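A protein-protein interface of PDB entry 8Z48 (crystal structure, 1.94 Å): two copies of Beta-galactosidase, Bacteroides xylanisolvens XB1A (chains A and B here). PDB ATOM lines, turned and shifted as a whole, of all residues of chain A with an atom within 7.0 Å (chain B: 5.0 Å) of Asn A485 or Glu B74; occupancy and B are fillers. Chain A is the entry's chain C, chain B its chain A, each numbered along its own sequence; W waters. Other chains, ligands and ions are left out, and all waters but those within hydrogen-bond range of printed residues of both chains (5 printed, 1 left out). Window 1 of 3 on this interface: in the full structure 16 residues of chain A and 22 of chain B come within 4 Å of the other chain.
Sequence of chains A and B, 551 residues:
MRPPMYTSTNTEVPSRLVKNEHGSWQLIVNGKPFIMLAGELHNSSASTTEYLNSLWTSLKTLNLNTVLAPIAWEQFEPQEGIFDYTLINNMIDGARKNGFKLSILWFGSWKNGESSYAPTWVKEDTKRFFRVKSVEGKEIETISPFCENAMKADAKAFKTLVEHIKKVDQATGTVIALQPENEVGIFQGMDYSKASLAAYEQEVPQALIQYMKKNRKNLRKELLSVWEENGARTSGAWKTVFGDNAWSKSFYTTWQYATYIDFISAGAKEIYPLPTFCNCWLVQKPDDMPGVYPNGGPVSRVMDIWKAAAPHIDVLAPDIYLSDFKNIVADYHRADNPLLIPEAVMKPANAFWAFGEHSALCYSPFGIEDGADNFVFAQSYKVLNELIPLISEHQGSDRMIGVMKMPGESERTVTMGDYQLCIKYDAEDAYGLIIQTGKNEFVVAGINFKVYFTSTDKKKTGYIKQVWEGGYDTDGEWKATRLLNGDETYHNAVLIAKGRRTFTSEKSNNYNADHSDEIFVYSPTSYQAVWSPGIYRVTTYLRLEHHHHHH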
ATOM      1  N   LYS A 465      17.202  18.244   9.411  1.00  0.00           N
ATOM      2  CA  LYS A 465      17.521  18.494   8.014  1.00  0.00           C
ATOM      3  C   LYS A 465      18.766  17.701   7.617  1.00  0.00           C
ATOM      4  O   LYS A 465      18.699  16.876   6.699  1.00  0.00           O
ATOM      5  CB  LYS A 465      17.674  19.986   7.685  1.00  0.00           C
ATOM      6  CG  LYS A 465      17.590  20.250   6.183  1.00  0.00           C
ATOM      7  CD  LYS A 465      18.131  21.597   5.711  1.00  0.00           C
ATOM      8  CE  LYS A 465      17.942  22.740   6.640  1.00  0.00           C
ATOM      9  NZ  LYS A 465      17.959  24.013   5.912  1.00  0.00           N
ATOM     10  N   GLN A 466      19.883  18.008   8.277  1.00  0.00           N
ATOM     11  CA  GLN A 466      21.123  17.235   8.207  1.00  0.00           C
ATOM     12  C   GLN A 466      21.796  17.128   9.582  1.00  0.00           C
ATOM     13  O   GLN A 466      21.541  17.960  10.442  1.00  0.00           O
ATOM     14  CB  GLN A 466      22.112  17.879   7.235  1.00  0.00           C
ATOM     15  CG  GLN A 466      21.562  17.988   5.819  1.00  0.00           C
ATOM     16  CD  GLN A 466      22.604  18.494   4.858  1.00  0.00           C
ATOM     17  OE1 GLN A 466      23.074  19.632   4.983  1.00  0.00           O
ATOM     18  NE2 GLN A 466      22.950  17.679   3.873  1.00  0.00           N
ATOM     19  N   VAL A 467      22.662  16.107   9.748  1.00  0.00           N
ATOM     20  CA  VAL A 467      23.490  15.853  10.934  1.00  0.00           C
ATOM     21  C   VAL A 467      24.945  15.614  10.499  1.00  0.00           C
ATOM     22  O   VAL A 467      25.220  14.874   9.540  1.00  0.00           O
ATOM     23  CB  VAL A 467      22.995  14.644  11.762  1.00  0.00           C
ATOM     24  CG1 VAL A 467      23.822  14.393  13.031  1.00  0.00           C
ATOM     25  CG2 VAL A 467      21.516  14.758  12.106  1.00  0.00           C
ATOM     26  N   TRP A 468      25.871  16.295  11.189  1.00  0.00           N
ATOM     27  CA  TRP A 468      27.291  16.015  11.071  1.00  0.00           C
ATOM     28  C   TRP A 468      27.855  15.721  12.466  1.00  0.00           C
ATOM     29  O   TRP A 468      27.489  16.353  13.457  1.00  0.00           O
ATOM     30  CB  TRP A 468      28.066  17.176  10.428  1.00  0.00           C
ATOM     31  CG  TRP A 468      27.598  17.652   9.074  1.00  0.00           C
ATOM     32  CD1 TRP A 468      28.121  17.371   7.841  1.00  0.00           C
ATOM     33  CD2 TRP A 468      26.525  18.583   8.854  1.00  0.00           C
ATOM     34  NE1 TRP A 468      27.430  18.046   6.864  1.00  0.00           N
ATOM     35  CE2 TRP A 468      26.441  18.794   7.457  1.00  0.00           C
ATOM     36  CE3 TRP A 468      25.632  19.255   9.702  1.00  0.00           C
ATOM     37  CZ2 TRP A 468      25.497  19.657   6.911  1.00  0.00           C
ATOM     38  CZ3 TRP A 468      24.694  20.101   9.156  1.00  0.00           C
ATOM     39  CH2 TRP A 468      24.626  20.293   7.773  1.00  0.00           C
ATOM     40  N   ARG A 482      31.949  12.935   9.822  1.00  0.00           N
ATOM     41  CA  ARG A 482      30.940  12.249   9.026  1.00  0.00           C
ATOM     42  C   ARG A 482      29.732  13.169   8.899  1.00  0.00           C
ATOM     43  O   ARG A 482      29.465  13.971   9.785  1.00  0.00           O
ATOM     44  CB  ARG A 482      30.543  10.890   9.610  1.00  0.00           C
ATOM     45  CG  ARG A 482      31.572   9.771   9.529  1.00  0.00           C
ATOM     46  CD  ARG A 482      31.090   8.431  10.128  1.00  0.00           C
ATOM     47  NE  ARG A 482      31.030   8.418  11.598  1.00  0.00           N
ATOM     48  CZ  ARG A 482      30.371   7.535  12.320  1.00  0.00           C
ATOM     49  NH1 ARG A 482      29.747   6.535  11.728  1.00  0.00           N
ATOM     50  NH2 ARG A 482      30.368   7.625  13.636  1.00  0.00           N
ATOM     51  N   LEU A 483      29.054  13.081   7.763  1.00  0.00           N
ATOM     52  CA  LEU A 483      27.647  13.424   7.687  1.00  0.00           C
ATOM     53  C   LEU A 483      26.927  12.153   8.132  1.00  0.00           C
ATOM     54  O   LEU A 483      27.123  11.112   7.537  1.00  0.00           O
ATOM     55  CB  LEU A 483      27.259  13.896   6.277  1.00  0.00           C
ATOM     56  CG  LEU A 483      25.922  14.643   6.168  1.00  0.00           C
ATOM     57  CD1 LEU A 483      25.842  15.413   4.880  1.00  0.00           C
ATOM     58  CD2 LEU A 483      24.706  13.674   6.300  1.00  0.00           C
ATOM     59  N   LEU A 484      26.203  12.196   9.249  1.00  0.00           N
ATOM     60  CA  LEU A 484      25.464  11.045   9.754  1.00  0.00           C
ATOM     61  C   LEU A 484      24.074  11.056   9.115  1.00  0.00           C
ATOM     62  O   LEU A 484      23.443  12.115   8.964  1.00  0.00           O
ATOM     63  CB  LEU A 484      25.347  11.021  11.285  1.00  0.00           C
ATOM     64  CG  LEU A 484      26.643  10.894  12.092  1.00  0.00           C
ATOM     65  CD1 LEU A 484      26.337  10.882  13.584  1.00  0.00           C
ATOM     66  CD2 LEU A 484      27.454   9.643  11.786  1.00  0.00           C
ATOM     67  N   ASN A 485      23.675   9.870   8.629  1.00  0.00           N
ATOM     68  CA  ASN A 485      22.388   9.670   7.983  1.00  0.00           C
ATOM     69  C   ASN A 485      22.114   8.159   7.981  1.00  0.00           C
ATOM     70  O   ASN A 485      22.910   7.378   8.516  1.00  0.00           O
ATOM     71  CB  ASN A 485      22.402  10.388   6.628  1.00  0.00           C
ATOM     72  CG  ASN A 485      21.042  10.771   6.121  1.00  0.00           C
ATOM     73  OD1 ASN A 485      20.022  10.177   6.491  1.00  0.00           O
ATOM     74  ND2 ASN A 485      21.020  11.721   5.214  1.00  0.00           N
ATOM     75  N   GLY A 486      20.982   7.758   7.388  1.00  0.00           N
ATOM     76  CA  GLY A 486      20.603   6.359   7.293  1.00  0.00           C
ATOM     77  C   GLY A 486      20.508   5.733   8.678  1.00  0.00           C
ATOM     78  O   GLY A 486      19.891   6.312   9.563  1.00  0.00           O
ATOM     79  N   ASP A 487      21.114   4.550   8.868  1.00  0.00           N
ATOM     80  CA  ASP A 487      21.073   3.901  10.168  1.00  0.00           C
ATOM     81  C   ASP A 487      21.558   4.866  11.248  1.00  0.00           C
ATOM     82  O   ASP A 487      21.030   4.829  12.361  1.00  0.00           O
ATOM     83  CB  ASP A 487      21.900   2.624  10.241  1.00  0.00           C
ATOM     84  CG  ASP A 487      21.519   1.519   9.272  1.00  0.00           C
ATOM     85  OD1 ASP A 487      20.373   1.551   8.792  1.00  0.00           O
ATOM     86  OD2 ASP A 487      22.402   0.686   8.966  1.00  0.00           O
ATOM     87  N   GLU A 488      22.533   5.736  10.929  1.00  0.00           N
ATOM     88  CA  GLU A 488      23.183   6.537  11.967  1.00  0.00           C
ATOM     89  C   GLU A 488      22.236   7.613  12.505  1.00  0.00           C
ATOM     90  O   GLU A 488      22.549   8.187  13.552  1.00  0.00           O
ATOM     91  CB  GLU A 488      24.557   7.105  11.564  1.00  0.00           C
ATOM     92  CG  GLU A 488      25.598   6.006  11.351  1.00  0.00           C
ATOM     93  CD  GLU A 488      25.406   5.017  10.218  1.00  0.00           C
ATOM     94  OE1 GLU A 488      25.306   5.469   9.052  1.00  0.00           O
ATOM     95  OE2 GLU A 488      25.355   3.787  10.492  1.00  0.00           O
ATOM     96  N   THR A 489      21.088   7.864  11.821  1.00  0.00           N
ATOM     97  CA  THR A 489      20.113   8.866  12.288  1.00  0.00           C
ATOM     98  C   THR A 489      18.666   8.357  12.210  1.00  0.00           C
ATOM     99  O   THR A 489      17.720   9.146  12.322  1.00  0.00           O
ATOM    100  CB  THR A 489      20.201  10.207  11.543  1.00  0.00           C
ATOM    101  OG1 THR A 489      19.899  10.021  10.162  1.00  0.00           O
ATOM    102  CG2 THR A 489      21.516  10.945  11.729  1.00  0.00           C
ATOM    103  N   TYR A 490      18.505   7.045  12.032  1.00  0.00           N
ATOM    104  CA  TYR A 490      17.237   6.446  11.652  1.00  0.00           C
ATOM    105  C   TYR A 490      16.544   7.300  10.590  1.00  0.00           C
ATOM    106  O   TYR A 490      15.424   7.763  10.846  1.00  0.00           O
ATOM    107  CB  TYR A 490      16.402   6.283  12.930  1.00  0.00           C
ATOM    108  CG  TYR A 490      16.864   5.264  13.962  1.00  0.00           C
ATOM    109  CD1 TYR A 490      17.809   4.301  13.647  1.00  0.00           C
ATOM    110  CD2 TYR A 490      16.310   5.228  15.240  1.00  0.00           C
ATOM    111  CE1 TYR A 490      18.232   3.367  14.577  1.00  0.00           C
ATOM    112  CE2 TYR A 490      16.713   4.283  16.176  1.00  0.00           C
ATOM    113  CZ  TYR A 490      17.677   3.354  15.838  1.00  0.00           C
ATOM    114  OH  TYR A 490      18.103   2.377  16.675  1.00  0.00           O
ATOM    115  N   HIS A 491      17.278   7.585   9.493  1.00  0.00           N
ATOM    116  CA  HIS A 491      16.786   8.278   8.300  1.00  0.00           C
ATOM    117  C   HIS A 491      16.242   9.656   8.695  1.00  0.00           C
ATOM    118  O   HIS A 491      15.216  10.106   8.205  1.00  0.00           O
ATOM    119  CB  HIS A 491      15.931   7.330   7.435  1.00  0.00           C
ATOM    120  CG  HIS A 491      16.665   6.050   7.134  1.00  0.00           C
ATOM    121  ND1 HIS A 491      16.683   5.000   8.034  1.00  0.00           N
ATOM    122  CD2 HIS A 491      17.494   5.690   6.130  1.00  0.00           C
ATOM    123  CE1 HIS A 491      17.470   4.044   7.573  1.00  0.00           C
ATOM    124  NE2 HIS A 491      17.992   4.446   6.431  1.00  0.00           N
ATOM    125  N   ASN A 492      17.018  10.294   9.588  1.00  0.00           N
ATOM    126  CA  ASN A 492      16.811  11.616  10.153  1.00  0.00           C
ATOM    127  C   ASN A 492      15.555  11.679  11.025  1.00  0.00           C
ATOM    128  O   ASN A 492      15.108  12.770  11.258  1.00  0.00           O
ATOM    129  CB  ASN A 492      16.892  12.723   9.111  1.00  0.00           C
ATOM    130  CG  ASN A 492      18.278  12.916   8.528  1.00  0.00           C
ATOM    131  OD1 ASN A 492      19.311  12.513   9.091  1.00  0.00           O
ATOM    132  ND2 ASN A 492      18.334  13.541   7.380  1.00  0.00           N
ATOM    133  N   ASN B  43      26.379   3.119   6.278  1.00  0.00           N
ATOM    134  CA  ASN B  43      25.748   4.151   5.476  1.00  0.00           C
ATOM    135  C   ASN B  43      26.571   5.443   5.480  1.00  0.00           C
ATOM    136  O   ASN B  43      26.646   6.097   4.440  1.00  0.00           O
ATOM    137  CB  ASN B  43      24.336   4.418   5.982  1.00  0.00           C
ATOM    138  CG  ASN B  43      23.344   3.294   5.801  1.00  0.00           C
ATOM    139  OD1 ASN B  43      22.324   3.295   6.501  1.00  0.00           O
ATOM    140  ND2 ASN B  43      23.560   2.381   4.853  1.00  0.00           N
ATOM    141  N   SER B  44      27.081   5.877   6.658  1.00  0.00           N
ATOM    142  CA  SER B  44      27.731   7.176   6.820  1.00  0.00           C
ATOM    143  C   SER B  44      29.272   7.130   6.643  1.00  0.00           C
ATOM    144  O   SER B  44      29.970   8.151   6.776  1.00  0.00           O
ATOM    145  CB  SER B  44      27.357   7.814   8.146  1.00  0.00           C
ATOM    146  OG  SER B  44      25.944   7.916   8.356  1.00  0.00           O
ATOM    147  N   ALA B  72      25.750  10.138  -1.904  1.00  0.00           N
ATOM    148  CA  ALA B  72      24.517  10.726  -1.422  1.00  0.00           C
ATOM    149  C   ALA B  72      24.206  11.980  -2.245  1.00  0.00           C
ATOM    150  O   ALA B  72      25.051  12.851  -2.388  1.00  0.00           O
ATOM    151  CB  ALA B  72      24.677  11.020   0.048  1.00  0.00           C
ATOM    152  N   TRP B  73      22.997  12.049  -2.801  1.00  0.00           N
ATOM    153  CA  TRP B  73      22.561  13.194  -3.588  1.00  0.00           C
ATOM    154  C   TRP B  73      22.786  14.486  -2.805  1.00  0.00           C
ATOM    155  O   TRP B  73      23.313  15.456  -3.348  1.00  0.00           O
ATOM    156  CB  TRP B  73      21.088  12.999  -3.959  1.00  0.00           C
ATOM    157  CG  TRP B  73      20.512  13.946  -4.988  1.00  0.00           C
ATOM    158  CD1 TRP B  73      21.162  14.846  -5.787  1.00  0.00           C
ATOM    159  CD2 TRP B  73      19.122  14.029  -5.359  1.00  0.00           C
ATOM    160  NE1 TRP B  73      20.269  15.506  -6.594  1.00  0.00           N
ATOM    161  CE2 TRP B  73      19.013  15.023  -6.361  1.00  0.00           C
ATOM    162  CE3 TRP B  73      17.970  13.368  -4.938  1.00  0.00           C
ATOM    163  CZ2 TRP B  73      17.792  15.359  -6.946  1.00  0.00           C
ATOM    164  CZ3 TRP B  73      16.768  13.685  -5.526  1.00  0.00           C
ATOM    165  CH2 TRP B  73      16.682  14.671  -6.517  1.00  0.00           C
ATOM    166  N   GLU B  74      22.427  14.486  -1.515  1.00  0.00           N
ATOM    167  CA  GLU B  74      22.544  15.685  -0.690  1.00  0.00           C
ATOM    168  C   GLU B  74      23.961  16.273  -0.738  1.00  0.00           C
ATOM    169  O   GLU B  74      24.105  17.482  -0.656  1.00  0.00           O
ATOM    170  CB  GLU B  74      22.097  15.529   0.771  1.00  0.00           C
ATOM    171  CG  GLU B  74      22.861  14.481   1.571  1.00  0.00           C
ATOM    172  CD  GLU B  74      22.366  14.224   2.989  1.00  0.00           C
ATOM    173  OE1 GLU B  74      21.615  15.080   3.541  1.00  0.00           O
ATOM    174  OE2 GLU B  74      22.811  13.181   3.557  1.00  0.00           O
ATOM    175  N   GLN B  75      24.993  15.437  -0.863  1.00  0.00           N
ATOM    176  CA  GLN B  75      26.367  15.924  -0.920  1.00  0.00           C
ATOM    177  C   GLN B  75      26.856  16.137  -2.346  1.00  0.00           C
ATOM    178  O   GLN B  75      27.703  17.003  -2.596  1.00  0.00           O
ATOM    179  CB  GLN B  75      27.330  14.925  -0.281  1.00  0.00           C
ATOM    180  CG  GLN B  75      26.990  14.638   1.170  1.00  0.00           C
ATOM    181  CD  GLN B  75      27.902  13.586   1.717  1.00  0.00           C
ATOM    182  OE1 GLN B  75      27.807  12.424   1.302  1.00  0.00           O
ATOM    183  NE2 GLN B  75      28.843  14.036   2.544  1.00  0.00           N
ATOM    184  N   PHE B  76      26.340  15.321  -3.273  1.00  0.00           N
ATOM    185  CA  PHE B  76      26.771  15.367  -4.661  1.00  0.00           C
ATOM    186  C   PHE B  76      26.229  16.613  -5.363  1.00  0.00           C
ATOM    187  O   PHE B  76      26.927  17.190  -6.202  1.00  0.00           O
ATOM    188  CB  PHE B  76      26.335  14.108  -5.403  1.00  0.00           C
ATOM    189  CG  PHE B  76      26.752  14.109  -6.865  1.00  0.00           C
ATOM    190  CD1 PHE B  76      28.089  14.007  -7.218  1.00  0.00           C
ATOM    191  CD2 PHE B  76      25.800  14.190  -7.873  1.00  0.00           C
ATOM    192  CE1 PHE B  76      28.469  13.996  -8.551  1.00  0.00           C
ATOM    193  CE2 PHE B  76      26.183  14.164  -9.198  1.00  0.00           C
ATOM    194  CZ  PHE B  76      27.519  14.083  -9.537  1.00  0.00           C
ATOM    195  N   GLU B  77      24.997  17.014  -5.028  1.00  0.00           N
ATOM    196  CA  GLU B  77      24.395  18.204  -5.608  1.00  0.00           C
ATOM    197  C   GLU B  77      23.833  19.066  -4.485  1.00  0.00           C
ATOM    198  O   GLU B  77      22.624  19.051  -4.240  1.00  0.00           O
ATOM    199  CB  GLU B  77      23.289  17.839  -6.587  1.00  0.00           C
ATOM    200  CG  GLU B  77      22.902  19.030  -7.460  1.00  0.00           C
ATOM    201  CD  GLU B  77      21.780  18.744  -8.427  1.00  0.00           C
ATOM    202  OE1 GLU B  77      21.168  17.654  -8.327  1.00  0.00           O
ATOM    203  OE2 GLU B  77      21.539  19.613  -9.287  1.00  0.00           O
ATOM    204  N   PRO B  78      24.704  19.776  -3.732  1.00  0.00           N
ATOM    205  CA  PRO B  78      24.282  20.426  -2.497  1.00  0.00           C
ATOM    206  C   PRO B  78      23.409  21.648  -2.764  1.00  0.00           C
ATOM    207  O   PRO B  78      22.584  21.993  -1.926  1.00  0.00           O
ATOM    208  CB  PRO B  78      25.613  20.777  -1.804  1.00  0.00           C
ATOM    209  CG  PRO B  78      26.629  20.902  -2.943  1.00  0.00           C
ATOM    210  CD  PRO B  78      26.144  19.933  -3.994  1.00  0.00           C
ATOM    211  N   PHE B 107      22.375   6.948  -3.222  1.00  0.00           N
ATOM    212  CA  PHE B 107      21.390   7.344  -2.225  1.00  0.00           C
ATOM    213  C   PHE B 107      20.764   8.671  -2.641  1.00  0.00           C
ATOM    214  O   PHE B 107      21.207   9.740  -2.210  1.00  0.00           O
ATOM    215  CB  PHE B 107      21.979   7.437  -0.815  1.00  0.00           C
ATOM    216  CG  PHE B 107      22.434   6.135  -0.170  1.00  0.00           C
ATOM    217  CD1 PHE B 107      22.187   4.900  -0.769  1.00  0.00           C
ATOM    218  CD2 PHE B 107      23.092   6.170   1.061  1.00  0.00           C
ATOM    219  CE1 PHE B 107      22.580   3.714  -0.146  1.00  0.00           C
ATOM    220  CE2 PHE B 107      23.479   4.992   1.689  1.00  0.00           C
ATOM    221  CZ  PHE B 107      23.259   3.768   1.071  1.00  0.00           C
ATOM    222  N   SER B 116      15.759  10.821   3.119  1.00  0.00           N
ATOM    223  CA  SER B 116      16.626  11.567   4.019  1.00  0.00           C
ATOM    224  C   SER B 116      17.937  11.986   3.333  1.00  0.00           C
ATOM    225  O   SER B 116      18.619  12.879   3.827  1.00  0.00           O
ATOM    226  CB  SER B 116      16.855  10.829   5.324  1.00  0.00           C
ATOM    227  OG  SER B 116      17.766   9.741   5.191  1.00  0.00           O
ATOM    228  N   TYR B 117      18.268  11.411   2.160  1.00  0.00           N
ATOM    229  CA  TYR B 117      19.471  11.811   1.454  1.00  0.00           C
ATOM    230  C   TYR B 117      19.184  12.749   0.276  1.00  0.00           C
ATOM    231  O   TYR B 117      20.095  13.115  -0.457  1.00  0.00           O
ATOM    232  CB  TYR B 117      20.222  10.587   0.944  1.00  0.00           C
ATOM    233  CG  TYR B 117      20.822   9.687   2.010  1.00  0.00           C
ATOM    234  CD1 TYR B 117      20.060   8.691   2.620  1.00  0.00           C
ATOM    235  CD2 TYR B 117      22.163   9.782   2.348  1.00  0.00           C
ATOM    236  CE1 TYR B 117      20.625   7.800   3.511  1.00  0.00           C
ATOM    237  CE2 TYR B 117      22.737   8.915   3.252  1.00  0.00           C
ATOM    238  CZ  TYR B 117      21.965   7.920   3.832  1.00  0.00           C
ATOM    239  OH  TYR B 117      22.511   7.006   4.676  1.00  0.00           O
ATOM    240  N   ALA B 118      17.935  13.178   0.120  1.00  0.00           N
ATOM    241  CA  ALA B 118      17.634  14.227  -0.838  1.00  0.00           C
ATOM    242  C   ALA B 118      18.274  15.538  -0.391  1.00  0.00           C
ATOM    243  O   ALA B 118      18.419  15.829   0.778  1.00  0.00           O
ATOM    244  CB  ALA B 118      16.137  14.340  -1.073  1.00  0.00           C
ATOM    245  N   PRO B 119      18.779  16.345  -1.342  1.00  0.00           N
ATOM    246  CA  PRO B 119      19.346  17.650  -1.011  1.00  0.00           C
ATOM    247  C   PRO B 119      18.393  18.525  -0.199  1.00  0.00           C
ATOM    248  O   PRO B 119      17.184  18.354  -0.265  1.00  0.00           O
ATOM    249  CB  PRO B 119      19.659  18.246  -2.387  1.00  0.00           C
ATOM    250  CG  PRO B 119      19.756  17.066  -3.345  1.00  0.00           C
ATOM    251  CD  PRO B 119      18.829  16.014  -2.777  1.00  0.00           C
ATOM    252  N   LYS B 123      14.286  18.823  -0.210  1.00  0.00           N
ATOM    253  CA  LYS B 123      13.474  18.653   0.983  1.00  0.00           C
ATOM    254  C   LYS B 123      12.590  19.887   1.223  1.00  0.00           C
ATOM    255  O   LYS B 123      11.410  19.765   1.563  1.00  0.00           O
ATOM    256  CB  LYS B 123      14.398  18.418   2.188  1.00  0.00           C
ATOM    257  CG  LYS B 123      15.104  17.065   2.215  1.00  0.00           C
ATOM    258  CD  LYS B 123      15.997  16.902   3.433  1.00  0.00           C
ATOM    259  CE  LYS B 123      16.695  15.580   3.456  1.00  0.00           C
ATOM    260  NZ  LYS B 123      17.707  15.570   4.500  1.00  0.00           N
HETATM  261  O   HOH W   1      24.549   7.929   5.852  1.00  0.00           O
HETATM  262  O   HOH W   2      19.759  16.860   2.936  1.00  0.00           O
HETATM  263  O   HOH W   3      24.933   1.910   8.511  1.00  0.00           O
HETATM  264  O   HOH W   4      15.641  15.117   6.567  1.00  0.00           O
HETATM  265  O   HOH W   5      25.367  18.302   2.002  1.00  0.00           O
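The backbone NH (N) of Gly A486 is in hydrogen-bond range of the side-chain hydroxyl (OH) of Tyr B117, at 3.2 Å. OE1 of Glu A488 is in hydrogen-bond range of OG of Ser B44 (2.6 Å). OE2 of Glu B74 sits at hydrogen-bond distance from ND2 of Asn A485, at 2.8 Å. NZ of Lys B123 sits at hydrogen-bond distance from O of Lys A465 (2.7 Å). The side-chain carboxylate (OE1) of Glu B74 lies within hydrogen-bond range of the side-chain amide nitrogen (NE2) of Gln A466 (2.9 Å). OG of Ser B44 lies within hydrogen-bond range of N of Asn A485 (3.0 Å). OD1 of Asn B43 is in hydrogen-bond range of N of Asp A487 (2.9 Å). OG of Ser B116 is in hydrogen-bond range of OD1 of Asn A485, at 2.6 Å.
N of Leu A484 is in hydrogen-bond range of O of Val A467. The backbone NH (N) of Glu B74 sits at hydrogen-bond distance from the backbone carbonyl oxygen (O) of Tyr B117 (2.9 Å). O of Ser B116 lies within hydrogen-bond range of NZ of Lys B123 (2.9 Å). The side-chain amide oxygen (OD1) of Asn A492 is in hydrogen-bond range of the side-chain hydroxyl (OG1) of Thr A489. The backbone carbonyl oxygen of Lys A465 lies within hydrogen-bond range of the side-chain amide nitrogen of Asn A492, at 3.4 Å. O of Gly A486 is in hydrogen-bond range of N of His A491.
Arg A482 touches Ser B44 (CD to O, 3.5 Å). Ser B44 touches Leu A483 (CB to O, 3.4 Å). Glu B74 touches Leu A483. Leu A483 touches Gln B75 (CD1 to CG, 3.96 Å). Ser B44 touches Leu A484. Asn A485 touches Tyr B117 (C to OH, 3.5 Å). CA of Gly A486 touches OD1 of Asn B43, at 3.6 Å. OE1 of Glu A488 touches CB of Asn B43, at 3.4 Å. His A491 touches Ser B116 (O to CB, 3.4 Å). Asn A492 touches Lys B123 (ND2 to NZ, 3.6 Å).
Of the printed residues of chain B, Arg A482 touches Ser B44. Of the printed residues of chain B, Leu A484 touches Ser B44. Printed residues of chain B within 4 Å of Asn A485: Ser B44, Glu B74, Ser B116 and Tyr B117. Of the printed residues of chain B, Glu A488 touches Asn B43 (3.4 Å) and Ser B44 (2.6 Å). Trp B73 touches none of the printed residues of chain A. Of the printed residues of chain A, Gln B75 touches Leu A483 (3.96 Å). Pro B78 touches none of the printed residues of chain A. Of the printed residues of chain A, Lys B123 touches Lys A465 and Asn A492. The nearest residue of chain A that does not touch Glu B74 is Lys A465 (4.7 Å).
Of the 15 printed residues of chain A, 11 touch a printed residue of chain B. Among the printed residues, no Asp or Glu carboxylate lies within 4 Å of a Lys or Arg side-chain nitrogen of the other chain.
No position is printed for both chains. Of the 19 pairs that touch across the chains among the printed residues, none has its exchanged pair printed and touching as well.
Water W1 lies within hydrogen-bond range of the side-chain hydroxyl of Tyr B117 (2.5 Å), the side-chain hydroxyl of Ser B44 (2.9 Å), the backbone carbonyl oxygen of Asn B43 (3.1 Å) and the backbone carbonyl oxygen of Asn A485 (3.2 Å). Water W2 lies within hydrogen-bond range of the side-chain carboxylate (OE1) of Glu B74 (2.6 Å), the backbone carbonyl oxygen (O) of Ala B118 (2.7 Å), the side-chain amino group (NZ) of Lys B123 (2.9 Å) and the side-chain amide nitrogen (NE2) of Gln A466 (3.4 Å). Water W3 lies within hydrogen-bond range of the side-chain carboxylate (OE2) of Glu A488 (2.8 Å), the side-chain carboxylate (OD2) of Asp A487 (2.8 Å) and the backbone NH (N) of Asn B43 (2.9 Å). Water W4 lies within hydrogen-bond range of NZ of Lys B123 (3.0 Å) and ND2 of Asn A492 (3.2 Å). Water W5 lies within hydrogen-bond range of O of Glu B74 (3.1 Å) and NE2 of Gln A466 (3.1 Å).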
